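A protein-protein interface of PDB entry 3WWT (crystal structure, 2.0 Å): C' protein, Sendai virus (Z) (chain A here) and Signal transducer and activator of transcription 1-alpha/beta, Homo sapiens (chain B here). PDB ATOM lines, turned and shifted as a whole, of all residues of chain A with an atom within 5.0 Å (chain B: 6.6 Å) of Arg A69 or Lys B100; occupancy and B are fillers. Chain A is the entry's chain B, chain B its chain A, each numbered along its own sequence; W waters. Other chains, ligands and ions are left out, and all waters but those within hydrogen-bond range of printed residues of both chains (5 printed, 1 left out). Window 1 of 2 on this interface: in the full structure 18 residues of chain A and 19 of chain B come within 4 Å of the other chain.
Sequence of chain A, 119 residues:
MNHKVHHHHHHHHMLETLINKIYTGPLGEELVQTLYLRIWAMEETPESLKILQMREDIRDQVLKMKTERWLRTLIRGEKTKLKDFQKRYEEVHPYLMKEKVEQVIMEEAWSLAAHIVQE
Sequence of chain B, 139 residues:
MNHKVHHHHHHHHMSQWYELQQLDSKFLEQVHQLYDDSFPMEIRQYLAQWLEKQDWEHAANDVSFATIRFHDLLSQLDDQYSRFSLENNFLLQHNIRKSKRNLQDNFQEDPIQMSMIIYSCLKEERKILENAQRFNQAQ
OH of Tyr A95 lies within hydrogen-bond range of O of His B71 (3.4 Å).
The side-chain amide nitrogen (NE2) of Gln B104 is in hydrogen-bond range of the backbone carbonyl oxygen (O) of Arg A69, at 3.0 Å.
The side-chain amide nitrogen (NE2) of Gln B108 sits at hydrogen-bond distance from the side-chain hydroxyl (OG1) of Thr A73 (2.8 Å).
O of His B71 is in hydrogen-bond range of NH1 of Arg A69, at 3.0 Å.
The side-chain carboxylate (OE2) of Glu A68 lies within salt-bridge range of the guanidinium group (NE) of Arg B101.
The side-chain carboxylate (OD2) of Asp B78 is in salt-bridge range of the side-chain amino group (NZ) of Lys A66 (2.8 Å).
Of the 22 printed residues of chain B, 11 touch a printed residue of chain A.
Along chain B the printed residues that touch a printed residue of chain A span positions 71 to 108.
Printed residues of chain A that touch a printed residue of chain B: Met A65, Lys A66, Glu A68, Arg A69, Trp A70, Arg A72, Thr A73 and Tyr A95.
Hydrophobic or aromatic side chains of chain A that line the printed part of chain B: Met A65, Trp A70 and Tyr A95.
Along chain A the printed residues that touch a printed residue of chain B span positions 65 to 95.
Ile B43 touches none of the printed residues of chain A.
Of the printed residues of chain A, His B71 touches Arg A69 (3.0 Å), Trp A70 (3.7 Å), Thr A73 (3.8 Å) and Tyr A95 (3.4 Å).
Printed residues of chain A within 4 Å of Leu B74: Arg A69.
Of chain A, only Met A65 and Arg A69 come within 4 Å of Lys B100.
Of the printed residues of chain A, Gln B108 touches Arg A72 (3.96 Å) and Thr A73 (2.8 Å).
The nearest residue of chain B that does not touch Arg A69 is Asp B72 (4.8 Å).
Water W1 lies within hydrogen-bond range of OH of Tyr A95 and OD1 of Asp B72.
Water W3 lies within hydrogen-bond range of the side-chain carboxylate (OE2) of Glu A102 (2.5 Å), the side-chain hydroxyl (OG) of Ser B75 (2.6 Å) and the side-chain amino group (NZ) of Lys A66 (3.4 Å).
Water W5 lies within hydrogen-bond range of NZ of Lys A66 (2.8 Å) and OG of Ser B75 (2.9 Å).
OE1 of Gln B108 sits at hydrogen-bond distance from NE2 of Gln B104, at 2.8 Å.
The indole nitrogen of Trp A70 lies within hydrogen-bond range of the side-chain carboxylate of Glu A102.
The guanidinium group (NH2) of Arg A69 is in salt-bridge range of the side-chain carboxylate (OE2) of Glu A102 (3.3 Å).
The guanidinium group of Arg B97 is in hydrogen-bond range of the side-chain hydroxyl of Tyr B81.
OE2 of Glu A68 is in salt-bridge range of NE of Arg A72.
Among the printed residues, pairs that only touch across the chains: Tyr A95 with Asp B72, Tyr A95 with Ser B75, Met A65 with Asp B78, Thr A73 with Gln B104, Lys A66 with Ser B75, Arg A69 with Leu B74, Arg A72 with Arg B101, Met A65 with Lys B100, Met A65 with Arg B97, Met A65 with Tyr B81, Arg A72 with Gln B104, Trp A70 with His B71, Thr A73 with His B71, Arg A69 with Ser B75, Arg A72 with Gln B108 and Arg A69 with Lys B100.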
ATOM      1  N   MET A  65     -15.772 -37.018  -7.376  1.00  0.00           N
ATOM      2  CA  MET A  65     -16.771 -35.991  -7.080  1.00  0.00           C
ATOM      3  C   MET A  65     -16.250 -34.604  -7.427  1.00  0.00           C
ATOM      4  O   MET A  65     -16.994 -33.759  -7.952  1.00  0.00           O
ATOM      5  CB  MET A  65     -17.153 -36.065  -5.608  1.00  0.00           C
ATOM      6  CG  MET A  65     -18.004 -37.292  -5.259  1.00  0.00           C
ATOM      7  SD  MET A  65     -18.060 -37.461  -3.488  1.00  0.00           S
ATOM      8  CE  MET A  65     -18.878 -35.901  -3.020  1.00  0.00           C
ATOM      9  N   LYS A  66     -14.973 -34.345  -7.123  1.00  0.00           N
ATOM     10  CA  LYS A  66     -14.397 -33.040  -7.440  1.00  0.00           C
ATOM     11  C   LYS A  66     -14.324 -32.836  -8.945  1.00  0.00           C
ATOM     12  O   LYS A  66     -14.584 -31.734  -9.441  1.00  0.00           O
ATOM     13  CB  LYS A  66     -13.023 -32.911  -6.778  1.00  0.00           C
ATOM     14  CG  LYS A  66     -13.133 -32.586  -5.296  1.00  0.00           C
ATOM     15  CD  LYS A  66     -11.789 -32.278  -4.645  1.00  0.00           C
ATOM     16  CE  LYS A  66     -11.976 -31.864  -3.185  1.00  0.00           C
ATOM     17  NZ  LYS A  66     -12.897 -30.665  -3.017  1.00  0.00           N
ATOM     18  N   THR A  67     -14.035 -33.899  -9.698  1.00  0.00           N
ATOM     19  CA  THR A  67     -14.067 -33.772 -11.150  1.00  0.00           C
ATOM     20  C   THR A  67     -15.481 -33.510 -11.655  1.00  0.00           C
ATOM     21  O   THR A  67     -15.680 -32.684 -12.552  1.00  0.00           O
ATOM     22  CB  THR A  67     -13.494 -35.022 -11.823  1.00  0.00           C
ATOM     23  OG1 THR A  67     -12.187 -35.310 -11.296  1.00  0.00           O
ATOM     24  CG2 THR A  67     -13.403 -34.789 -13.332  1.00  0.00           C
ATOM     25  N   GLU A  68     -16.475 -34.198 -11.092  1.00  0.00           N
ATOM     26  CA  GLU A  68     -17.857 -33.987 -11.525  1.00  0.00           C
ATOM     27  C   GLU A  68     -18.291 -32.541 -11.297  1.00  0.00           C
ATOM     28  O   GLU A  68     -19.009 -31.962 -12.123  1.00  0.00           O
ATOM     29  CB  GLU A  68     -18.801 -34.949 -10.788  1.00  0.00           C
ATOM     30  CG  GLU A  68     -20.272 -34.732 -11.116  1.00  0.00           C
ATOM     31  CD  GLU A  68     -21.231 -35.538 -10.240  1.00  0.00           C
ATOM     32  OE1 GLU A  68     -20.769 -36.253  -9.331  1.00  0.00           O
ATOM     33  OE2 GLU A  68     -22.457 -35.452 -10.475  1.00  0.00           O
ATOM     34  N   ARG A  69     -17.876 -31.948 -10.173  1.00  0.00           N
ATOM     35  CA  ARG A  69     -18.227 -30.555  -9.886  1.00  0.00           C
ATOM     36  C   ARG A  69     -17.783 -29.626 -11.009  1.00  0.00           C
ATOM     37  O   ARG A  69     -18.520 -28.712 -11.398  1.00  0.00           O
ATOM     38  CB  ARG A  69     -17.619 -30.114  -8.554  1.00  0.00           C
ATOM     39  CG  ARG A  69     -18.175 -28.748  -8.037  1.00  0.00           C
ATOM     40  CD  ARG A  69     -17.205 -27.572  -8.318  1.00  0.00           C
ATOM     41  NE  ARG A  69     -16.037 -27.666  -7.440  1.00  0.00           N
ATOM     42  CZ  ARG A  69     -15.811 -26.908  -6.372  1.00  0.00           C
ATOM     43  NH1 ARG A  69     -16.651 -25.944  -6.026  1.00  0.00           N
ATOM     44  NH2 ARG A  69     -14.737 -27.134  -5.632  1.00  0.00           N
ATOM     45  N   TRP A  70     -16.587 -29.849 -11.557  1.00  0.00           N
ATOM     46  CA  TRP A  70     -16.104 -28.981 -12.627  1.00  0.00           C
ATOM     47  C   TRP A  70     -16.731 -29.319 -13.973  1.00  0.00           C
ATOM     48  O   TRP A  70     -16.985 -28.413 -14.771  1.00  0.00           O
ATOM     49  CB  TRP A  70     -14.569 -29.025 -12.691  1.00  0.00           C
ATOM     50  CG  TRP A  70     -13.952 -28.408 -11.446  1.00  0.00           C
ATOM     51  CD1 TRP A  70     -12.976 -28.947 -10.656  1.00  0.00           C
ATOM     52  CD2 TRP A  70     -14.322 -27.161 -10.827  1.00  0.00           C
ATOM     53  NE1 TRP A  70     -12.696 -28.102  -9.604  1.00  0.00           N
ATOM     54  CE2 TRP A  70     -13.512 -27.002  -9.688  1.00  0.00           C
ATOM     55  CE3 TRP A  70     -15.249 -26.154 -11.137  1.00  0.00           C
ATOM     56  CZ2 TRP A  70     -13.613 -25.886  -8.849  1.00  0.00           C
ATOM     57  CZ3 TRP A  70     -15.343 -25.045 -10.298  1.00  0.00           C
ATOM     58  CH2 TRP A  70     -14.534 -24.923  -9.177  1.00  0.00           C
ATOM     59  N   LEU A  71     -17.003 -30.599 -14.238  1.00  0.00           N
ATOM     60  CA  LEU A  71     -17.730 -30.965 -15.453  1.00  0.00           C
ATOM     61  C   LEU A  71     -19.092 -30.272 -15.505  1.00  0.00           C
ATOM     62  O   LEU A  71     -19.462 -29.678 -16.526  1.00  0.00           O
ATOM     63  CB  LEU A  71     -17.897 -32.481 -15.523  1.00  0.00           C
ATOM     64  CG  LEU A  71     -16.677 -33.295 -15.956  1.00  0.00           C
ATOM     65  CD1 LEU A  71     -16.947 -34.779 -15.734  1.00  0.00           C
ATOM     66  CD2 LEU A  71     -16.342 -33.036 -17.407  1.00  0.00           C
ATOM     67  N   ARG A  72     -19.846 -30.324 -14.401  1.00  0.00           N
ATOM     68  CA  ARG A  72     -21.131 -29.632 -14.319  1.00  0.00           C
ATOM     69  C   ARG A  72     -20.974 -28.121 -14.294  1.00  0.00           C
ATOM     70  O   ARG A  72     -21.951 -27.401 -14.528  1.00  0.00           O
ATOM     71  CB  ARG A  72     -21.905 -30.092 -13.077  1.00  0.00           C
ATOM     72  CG  ARG A  72     -22.165 -31.607 -13.034  1.00  0.00           C
ATOM     73  CD  ARG A  72     -23.233 -31.953 -12.000  1.00  0.00           C
ATOM     74  NE  ARG A  72     -23.553 -33.376 -11.995  1.00  0.00           N
ATOM     75  CZ  ARG A  72     -24.350 -33.972 -12.880  1.00  0.00           C
ATOM     76  NH1 ARG A  72     -24.919 -33.276 -13.860  1.00  0.00           N
ATOM     77  NH2 ARG A  72     -24.576 -35.272 -12.787  1.00  0.00           N
ATOM     78  N   THR A  73     -19.781 -27.617 -13.991  1.00  0.00           N
ATOM     79  CA  THR A  73     -19.541 -26.188 -14.147  1.00  0.00           C
ATOM     80  C   THR A  73     -19.352 -25.822 -15.617  1.00  0.00           C
ATOM     81  O   THR A  73     -19.882 -24.804 -16.076  1.00  0.00           O
ATOM     82  CB  THR A  73     -18.318 -25.759 -13.331  1.00  0.00           C
ATOM     83  OG1 THR A  73     -18.591 -25.900 -11.929  1.00  0.00           O
ATOM     84  CG2 THR A  73     -17.961 -24.295 -13.621  1.00  0.00           C
ATOM     85  N   TYR A  95     -11.803 -18.319  -7.830  1.00  0.00           N
ATOM     86  CA  TYR A  95     -11.882 -19.415  -6.873  1.00  0.00           C
ATOM     87  C   TYR A  95     -10.683 -20.350  -7.032  1.00  0.00           C
ATOM     88  O   TYR A  95     -10.013 -20.688  -6.052  1.00  0.00           O
ATOM     89  CB  TYR A  95     -13.206 -20.180  -7.045  1.00  0.00           C
ATOM     90  CG  TYR A  95     -13.297 -21.399  -6.153  1.00  0.00           C
ATOM     91  CD1 TYR A  95     -13.625 -21.278  -4.804  1.00  0.00           C
ATOM     92  CD2 TYR A  95     -13.027 -22.667  -6.654  1.00  0.00           C
ATOM     93  CE1 TYR A  95     -13.682 -22.404  -3.974  1.00  0.00           C
ATOM     94  CE2 TYR A  95     -13.073 -23.805  -5.833  1.00  0.00           C
ATOM     95  CZ  TYR A  95     -13.399 -23.662  -4.501  1.00  0.00           C
ATOM     96  OH  TYR A  95     -13.453 -24.775  -3.685  1.00  0.00           O
ATOM     97  N   GLU A 102      -7.904 -27.631  -6.759  1.00  0.00           N
ATOM     98  CA  GLU A 102      -9.058 -27.566  -7.660  1.00  0.00           C
ATOM     99  C   GLU A 102      -8.648 -27.115  -9.050  1.00  0.00           C
ATOM    100  O   GLU A 102      -9.296 -27.476 -10.040  1.00  0.00           O
ATOM    101  CB  GLU A 102     -10.131 -26.605  -7.119  1.00  0.00           C
ATOM    102  CG  GLU A 102     -10.726 -26.954  -5.748  1.00  0.00           C
ATOM    103  CD  GLU A 102     -11.595 -28.217  -5.758  1.00  0.00           C
ATOM    104  OE1 GLU A 102     -11.907 -28.752  -6.839  1.00  0.00           O
ATOM    105  OE2 GLU A 102     -11.964 -28.669  -4.663  1.00  0.00           O
ATOM    106  N   ILE B  43     -27.970 -29.826   4.509  1.00  0.00           N
ATOM    107  CA  ILE B  43     -26.737 -29.055   4.369  1.00  0.00           C
ATOM    108  C   ILE B  43     -26.602 -28.066   5.516  1.00  0.00           C
ATOM    109  O   ILE B  43     -25.512 -27.880   6.070  1.00  0.00           O
ATOM    110  CB  ILE B  43     -26.703 -28.352   3.005  1.00  0.00           C
ATOM    111  CG1 ILE B  43     -26.785 -29.370   1.881  1.00  0.00           C
ATOM    112  CG2 ILE B  43     -25.446 -27.491   2.860  1.00  0.00           C
ATOM    113  CD1 ILE B  43     -27.026 -28.715   0.542  1.00  0.00           C
ATOM    114  N   PHE B  70     -20.143 -19.959  -3.057  1.00  0.00           N
ATOM    115  CA  PHE B  70     -20.892 -21.076  -3.634  1.00  0.00           C
ATOM    116  C   PHE B  70     -19.971 -22.271  -3.875  1.00  0.00           C
ATOM    117  O   PHE B  70     -20.266 -23.405  -3.475  1.00  0.00           O
ATOM    118  CB  PHE B  70     -21.556 -20.608  -4.933  1.00  0.00           C
ATOM    119  CG  PHE B  70     -22.160 -21.716  -5.765  1.00  0.00           C
ATOM    120  CD1 PHE B  70     -23.391 -22.265  -5.435  1.00  0.00           C
ATOM    121  CD2 PHE B  70     -21.519 -22.175  -6.900  1.00  0.00           C
ATOM    122  CE1 PHE B  70     -23.960 -23.280  -6.209  1.00  0.00           C
ATOM    123  CE2 PHE B  70     -22.088 -23.202  -7.685  1.00  0.00           C
ATOM    124  CZ  PHE B  70     -23.309 -23.745  -7.333  1.00  0.00           C
ATOM    125  N   HIS B  71     -18.819 -22.020  -4.493  1.00  0.00           N
ATOM    126  CA  HIS B  71     -17.874 -23.101  -4.731  1.00  0.00           C
ATOM    127  C   HIS B  71     -17.149 -23.534  -3.465  1.00  0.00           C
ATOM    128  O   HIS B  71     -16.801 -24.716  -3.340  1.00  0.00           O
ATOM    129  CB  HIS B  71     -16.910 -22.684  -5.831  1.00  0.00           C
ATOM    130  CG  HIS B  71     -17.554 -22.718  -7.172  1.00  0.00           C
ATOM    131  ND1 HIS B  71     -17.928 -23.900  -7.774  1.00  0.00           N
ATOM    132  CD2 HIS B  71     -17.975 -21.725  -7.991  1.00  0.00           C
ATOM    133  CE1 HIS B  71     -18.513 -23.633  -8.927  1.00  0.00           C
ATOM    134  NE2 HIS B  71     -18.554 -22.320  -9.082  1.00  0.00           N
ATOM    135  N   ASP B  72     -16.940 -22.622  -2.512  1.00  0.00           N
ATOM    136  CA  ASP B  72     -16.480 -23.037  -1.187  1.00  0.00           C
ATOM    137  C   ASP B  72     -17.441 -24.045  -0.571  1.00  0.00           C
ATOM    138  O   ASP B  72     -17.023 -25.010   0.085  1.00  0.00           O
ATOM    139  CB  ASP B  72     -16.381 -21.844  -0.234  1.00  0.00           C
ATOM    140  CG  ASP B  72     -15.140 -20.981  -0.435  1.00  0.00           C
ATOM    141  OD1 ASP B  72     -14.153 -21.420  -1.056  1.00  0.00           O
ATOM    142  OD2 ASP B  72     -15.168 -19.829   0.065  1.00  0.00           O
ATOM    143  N   LEU B  73     -18.740 -23.790  -0.704  1.00  0.00           N
ATOM    144  CA  LEU B  73     -19.722 -24.670  -0.085  1.00  0.00           C
ATOM    145  C   LEU B  73     -19.650 -26.071  -0.689  1.00  0.00           C
ATOM    146  O   LEU B  73     -19.684 -27.065   0.034  1.00  0.00           O
ATOM    147  CB  LEU B  73     -21.126 -24.060  -0.238  1.00  0.00           C
ATOM    148  CG  LEU B  73     -22.210 -24.613   0.695  1.00  0.00           C
ATOM    149  CD1 LEU B  73     -23.373 -23.635   0.859  1.00  0.00           C
ATOM    150  CD2 LEU B  73     -22.712 -25.951   0.170  1.00  0.00           C
ATOM    151  N   LEU B  74     -19.552 -26.164  -2.012  1.00  0.00           N
ATOM    152  CA  LEU B  74     -19.431 -27.473  -2.651  1.00  0.00           C
ATOM    153  C   LEU B  74     -18.195 -28.222  -2.169  1.00  0.00           C
ATOM    154  O   LEU B  74     -18.237 -29.439  -1.963  1.00  0.00           O
ATOM    155  CB  LEU B  74     -19.393 -27.300  -4.161  1.00  0.00           C
ATOM    156  CG  LEU B  74     -20.698 -26.695  -4.653  1.00  0.00           C
ATOM    157  CD1 LEU B  74     -20.591 -26.364  -6.120  1.00  0.00           C
ATOM    158  CD2 LEU B  74     -21.826 -27.711  -4.392  1.00  0.00           C
ATOM    159  N   SER B  75     -17.078 -27.514  -1.991  1.00  0.00           N
ATOM    160  CA  SER B  75     -15.881 -28.174  -1.487  1.00  0.00           C
ATOM    161  C   SER B  75     -16.027 -28.566  -0.023  1.00  0.00           C
ATOM    162  O   SER B  75     -15.498 -29.608   0.386  1.00  0.00           O
ATOM    163  CB  SER B  75     -14.652 -27.271  -1.686  1.00  0.00           C
ATOM    164  OG  SER B  75     -13.546 -27.814  -0.981  1.00  0.00           O
ATOM    165  N   LEU B  77     -18.747 -29.651   1.200  1.00  0.00           N
ATOM    166  CA  LEU B  77     -19.514 -30.895   1.138  1.00  0.00           C
ATOM    167  C   LEU B  77     -18.619 -32.084   0.791  1.00  0.00           C
ATOM    168  O   LEU B  77     -18.873 -33.202   1.252  1.00  0.00           O
ATOM    169  CB  LEU B  77     -20.654 -30.764   0.125  1.00  0.00           C
ATOM    170  CG  LEU B  77     -21.828 -29.864   0.546  1.00  0.00           C
ATOM    171  CD1 LEU B  77     -22.836 -29.656  -0.607  1.00  0.00           C
ATOM    172  CD2 LEU B  77     -22.503 -30.416   1.782  1.00  0.00           C
ATOM    173  N   ASP B  78     -17.562 -31.870   0.000  1.00  0.00           N
ATOM    174  CA  ASP B  78     -16.576 -32.939  -0.210  1.00  0.00           C
ATOM    175  C   ASP B  78     -15.896 -33.323   1.096  1.00  0.00           C
ATOM    176  O   ASP B  78     -15.641 -34.508   1.344  1.00  0.00           O
ATOM    177  CB  ASP B  78     -15.515 -32.526  -1.234  1.00  0.00           C
ATOM    178  CG  ASP B  78     -16.077 -32.301  -2.636  1.00  0.00           C
ATOM    179  OD1 ASP B  78     -17.058 -32.978  -3.031  1.00  0.00           O
ATOM    180  OD2 ASP B  78     -15.522 -31.435  -3.371  1.00  0.00           O
ATOM    181  N   TYR B  81     -18.335 -35.381   2.999  1.00  0.00           N
ATOM    182  CA  TYR B  81     -18.367 -36.704   2.398  1.00  0.00           C
ATOM    183  C   TYR B  81     -17.228 -37.587   2.900  1.00  0.00           C
ATOM    184  O   TYR B  81     -17.441 -38.758   3.235  1.00  0.00           O
ATOM    185  CB  TYR B  81     -18.316 -36.579   0.877  1.00  0.00           C
ATOM    186  CG  TYR B  81     -18.378 -37.913   0.170  1.00  0.00           C
ATOM    187  CD1 TYR B  81     -17.225 -38.668  -0.030  1.00  0.00           C
ATOM    188  CD2 TYR B  81     -19.586 -38.420  -0.297  1.00  0.00           C
ATOM    189  CE1 TYR B  81     -17.274 -39.889  -0.670  1.00  0.00           C
ATOM    190  CE2 TYR B  81     -19.641 -39.641  -0.959  1.00  0.00           C
ATOM    191  CZ  TYR B  81     -18.480 -40.373  -1.134  1.00  0.00           C
ATOM    192  OH  TYR B  81     -18.514 -41.587  -1.781  1.00  0.00           O
ATOM    193  N   ASN B  95     -26.376 -39.050   0.078  1.00  0.00           N
ATOM    194  CA  ASN B  95     -27.101 -37.793   0.241  1.00  0.00           C
ATOM    195  C   ASN B  95     -26.204 -36.579  -0.026  1.00  0.00           C
ATOM    196  O   ASN B  95     -26.635 -35.611  -0.661  1.00  0.00           O
ATOM    197  CB  ASN B  95     -27.698 -37.744   1.641  1.00  0.00           C
ATOM    198  CG  ASN B  95     -28.928 -38.634   1.771  1.00  0.00           C
ATOM    199  OD1 ASN B  95     -29.421 -39.182   0.779  1.00  0.00           O
ATOM    200  ND2 ASN B  95     -29.435 -38.768   2.989  1.00  0.00           N
ATOM    201  N   ILE B  96     -24.947 -36.621   0.425  1.00  0.00           N
ATOM    202  CA  ILE B  96     -24.039 -35.507   0.133  1.00  0.00           C
ATOM    203  C   ILE B  96     -23.910 -35.324  -1.368  1.00  0.00           C
ATOM    204  O   ILE B  96     -23.970 -34.201  -1.879  1.00  0.00           O
ATOM    205  CB  ILE B  96     -22.666 -35.730   0.800  1.00  0.00           C
ATOM    206  CG1 ILE B  96     -22.766 -35.609   2.319  1.00  0.00           C
ATOM    207  CG2 ILE B  96     -21.607 -34.731   0.232  1.00  0.00           C
ATOM    208  CD1 ILE B  96     -23.193 -34.229   2.759  1.00  0.00           C
ATOM    209  N   ARG B  97     -23.778 -36.425  -2.112  1.00  0.00           N
ATOM    210  CA  ARG B  97     -23.601 -36.310  -3.554  1.00  0.00           C
ATOM    211  C   ARG B  97     -24.848 -35.747  -4.218  1.00  0.00           C
ATOM    212  O   ARG B  97     -24.750 -34.902  -5.115  1.00  0.00           O
ATOM    213  CB  ARG B  97     -23.218 -37.671  -4.151  1.00  0.00           C
ATOM    214  CG  ARG B  97     -21.701 -37.909  -4.088  1.00  0.00           C
ATOM    215  CD  ARG B  97     -21.266 -39.367  -3.938  1.00  0.00           C
ATOM    216  NE  ARG B  97     -21.379 -40.126  -5.160  1.00  0.00           N
ATOM    217  CZ  ARG B  97     -20.599 -41.158  -5.489  1.00  0.00           C
ATOM    218  NH1 ARG B  97     -19.600 -41.555  -4.703  1.00  0.00           N
ATOM    219  NH2 ARG B  97     -20.814 -41.784  -6.624  1.00  0.00           N
ATOM    220  N   LYS B  98     -26.026 -36.218  -3.798  1.00  0.00           N
ATOM    221  CA  LYS B  98     -27.283 -35.637  -4.267  1.00  0.00           C
ATOM    222  C   LYS B  98     -27.371 -34.151  -3.911  1.00  0.00           C
ATOM    223  O   LYS B  98     -27.740 -33.317  -4.749  1.00  0.00           O
ATOM    224  CB  LYS B  98     -28.454 -36.428  -3.658  1.00  0.00           C
ATOM    225  CG  LYS B  98     -29.853 -35.942  -4.029  1.00  0.00           C
ATOM    226  CD  LYS B  98     -30.932 -36.971  -3.615  1.00  0.00           C
ATOM    227  CE  LYS B  98     -30.822 -37.385  -2.145  1.00  0.00           C
ATOM    228  NZ  LYS B  98     -31.594 -36.481  -1.222  1.00  0.00           N
ATOM    229  N   SER B  99     -27.022 -33.801  -2.671  1.00  0.00           N
ATOM    230  CA  SER B  99     -27.051 -32.393  -2.253  1.00  0.00           C
ATOM    231  C   SER B  99     -26.215 -31.511  -3.179  1.00  0.00           C
ATOM    232  O   SER B  99     -26.667 -30.442  -3.615  1.00  0.00           O
ATOM    233  CB  SER B  99     -26.556 -32.258  -0.815  1.00  0.00           C
ATOM    234  OG  SER B  99     -27.470 -32.825   0.102  1.00  0.00           O
ATOM    235  N   LYS B 100     -24.989 -31.944  -3.490  1.00  0.00           N
ATOM    236  CA  LYS B 100     -24.110 -31.158  -4.356  1.00  0.00           C
ATOM    237  C   LYS B 100     -24.729 -30.955  -5.723  1.00  0.00           C
ATOM    238  O   LYS B 100     -24.729 -29.839  -6.257  1.00  0.00           O
ATOM    239  CB  LYS B 100     -22.742 -31.852  -4.526  1.00  0.00           C
ATOM    240  CG  LYS B 100     -21.836 -31.813  -3.313  1.00  0.00           C
ATOM    241  CD  LYS B 100     -20.423 -32.321  -3.662  1.00  0.00           C
ATOM    242  CE  LYS B 100     -19.677 -31.351  -4.586  1.00  0.00           C
ATOM    243  NZ  LYS B 100     -18.444 -32.004  -5.171  1.00  0.00           N
ATOM    244  N   ARG B 101     -25.204 -32.045  -6.336  1.00  0.00           N
ATOM    245  CA  ARG B 101     -25.843 -31.957  -7.645  1.00  0.00           C
ATOM    246  C   ARG B 101     -27.005 -30.971  -7.631  1.00  0.00           C
ATOM    247  O   ARG B 101     -27.129 -30.127  -8.526  1.00  0.00           O
ATOM    248  CB  ARG B 101     -26.332 -33.341  -8.081  1.00  0.00           C
ATOM    249  CG  ARG B 101     -25.370 -34.082  -8.981  1.00  0.00           C
ATOM    250  CD  ARG B 101     -25.564 -35.599  -8.852  1.00  0.00           C
ATOM    251  NE  ARG B 101     -24.288 -36.312  -8.738  1.00  0.00           N
ATOM    252  CZ  ARG B 101     -24.163 -37.566  -8.307  1.00  0.00           C
ATOM    253  NH1 ARG B 101     -25.244 -38.253  -7.944  1.00  0.00           N
ATOM    254  NH2 ARG B 101     -22.958 -38.129  -8.224  1.00  0.00           N
ATOM    255  N   ASN B 102     -27.874 -31.071  -6.628  1.00  0.00           N
ATOM    256  CA  ASN B 102     -29.049 -30.204  -6.594  1.00  0.00           C
ATOM    257  C   ASN B 102     -28.650 -28.737  -6.445  1.00  0.00           C
ATOM    258  O   ASN B 102     -29.185 -27.865  -7.148  1.00  0.00           O
ATOM    259  CB  ASN B 102     -29.986 -30.647  -5.466  1.00  0.00           C
ATOM    260  CG  ASN B 102     -30.632 -32.004  -5.745  1.00  0.00           C
ATOM    261  OD1 ASN B 102     -30.686 -32.447  -6.890  1.00  0.00           O
ATOM    262  ND2 ASN B 102     -31.125 -32.661  -4.705  1.00  0.00           N
ATOM    263  N   LEU B 103     -27.691 -28.446  -5.557  1.00  0.00           N
ATOM    264  CA  LEU B 103     -27.228 -27.064  -5.395  1.00  0.00           C
ATOM    265  C   LEU B 103     -26.706 -26.498  -6.704  1.00  0.00           C
ATOM    266  O   LEU B 103     -26.998 -25.348  -7.055  1.00  0.00           O
ATOM    267  CB  LEU B 103     -26.128 -26.982  -4.340  1.00  0.00           C
ATOM    268  CG  LEU B 103     -26.487 -26.804  -2.870  1.00  0.00           C
ATOM    269  CD1 LEU B 103     -25.206 -26.678  -2.084  1.00  0.00           C
ATOM    270  CD2 LEU B 103     -27.362 -25.588  -2.618  1.00  0.00           C
ATOM    271  N   GLN B 104     -25.919 -27.292  -7.437  1.00  0.00           N
ATOM    272  CA  GLN B 104     -25.376 -26.830  -8.708  1.00  0.00           C
ATOM    273  C   GLN B 104     -26.480 -26.606  -9.735  1.00  0.00           C
ATOM    274  O   GLN B 104     -26.488 -25.596 -10.444  1.00  0.00           O
ATOM    275  CB  GLN B 104     -24.351 -27.839  -9.229  1.00  0.00           C
ATOM    276  CG  GLN B 104     -22.960 -27.630  -8.669  1.00  0.00           C
ATOM    277  CD  GLN B 104     -21.886 -28.397  -9.436  1.00  0.00           C
ATOM    278  OE1 GLN B 104     -21.679 -29.580  -9.201  1.00  0.00           O
ATOM    279  NE2 GLN B 104     -21.186 -27.710 -10.334  1.00  0.00           N
ATOM    280  N   ASP B 105     -27.397 -27.563  -9.865  1.00  0.00           N
ATOM    281  CA  ASP B 105     -28.577 -27.355 -10.699  1.00  0.00           C
ATOM    282  C   ASP B 105     -29.314 -26.077 -10.313  1.00  0.00           C
ATOM    283  O   ASP B 105     -29.653 -25.250 -11.171  1.00  0.00           O
ATOM    284  CB  ASP B 105     -29.521 -28.552 -10.568  1.00  0.00           C
ATOM    285  CG  ASP B 105     -29.035 -29.767 -11.323  1.00  0.00           C
ATOM    286  OD1 ASP B 105     -29.513 -30.881 -10.997  1.00  0.00           O
ATOM    287  OD2 ASP B 105     -28.187 -29.612 -12.232  1.00  0.00           O
ATOM    288  N   GLN B 108     -26.235 -22.522  -9.658  1.00  0.00           N
ATOM    289  CA  GLN B 108     -25.002 -22.119 -10.326  1.00  0.00           C
ATOM    290  C   GLN B 108     -25.215 -21.030 -11.370  1.00  0.00           C
ATOM    291  O   GLN B 108     -24.269 -20.294 -11.676  1.00  0.00           O
ATOM    292  CB  GLN B 108     -24.306 -23.312 -10.975  1.00  0.00           C
ATOM    293  CG  GLN B 108     -22.832 -23.041 -11.193  1.00  0.00           C
ATOM    294  CD  GLN B 108     -22.000 -24.306 -11.233  1.00  0.00           C
ATOM    295  OE1 GLN B 108     -22.526 -25.422 -11.151  1.00  0.00           O
ATOM    296  NE2 GLN B 108     -20.692 -24.137 -11.361  1.00  0.00           N
HETATM  297  O   HOH W   1     -13.057 -24.122  -1.349  1.00  0.00           O
HETATM  298  O   HOH W   2     -16.315 -30.338  -5.514  1.00  0.00           O
HETATM  299  O   HOH W   3     -11.486 -27.607  -2.491  1.00  0.00           O
HETATM  300  O   HOH W   4     -19.596 -33.653  -7.082  1.00  0.00           O
HETATM  301  O   HOH W   5     -12.499 -30.417  -0.262  1.00  0.00           O
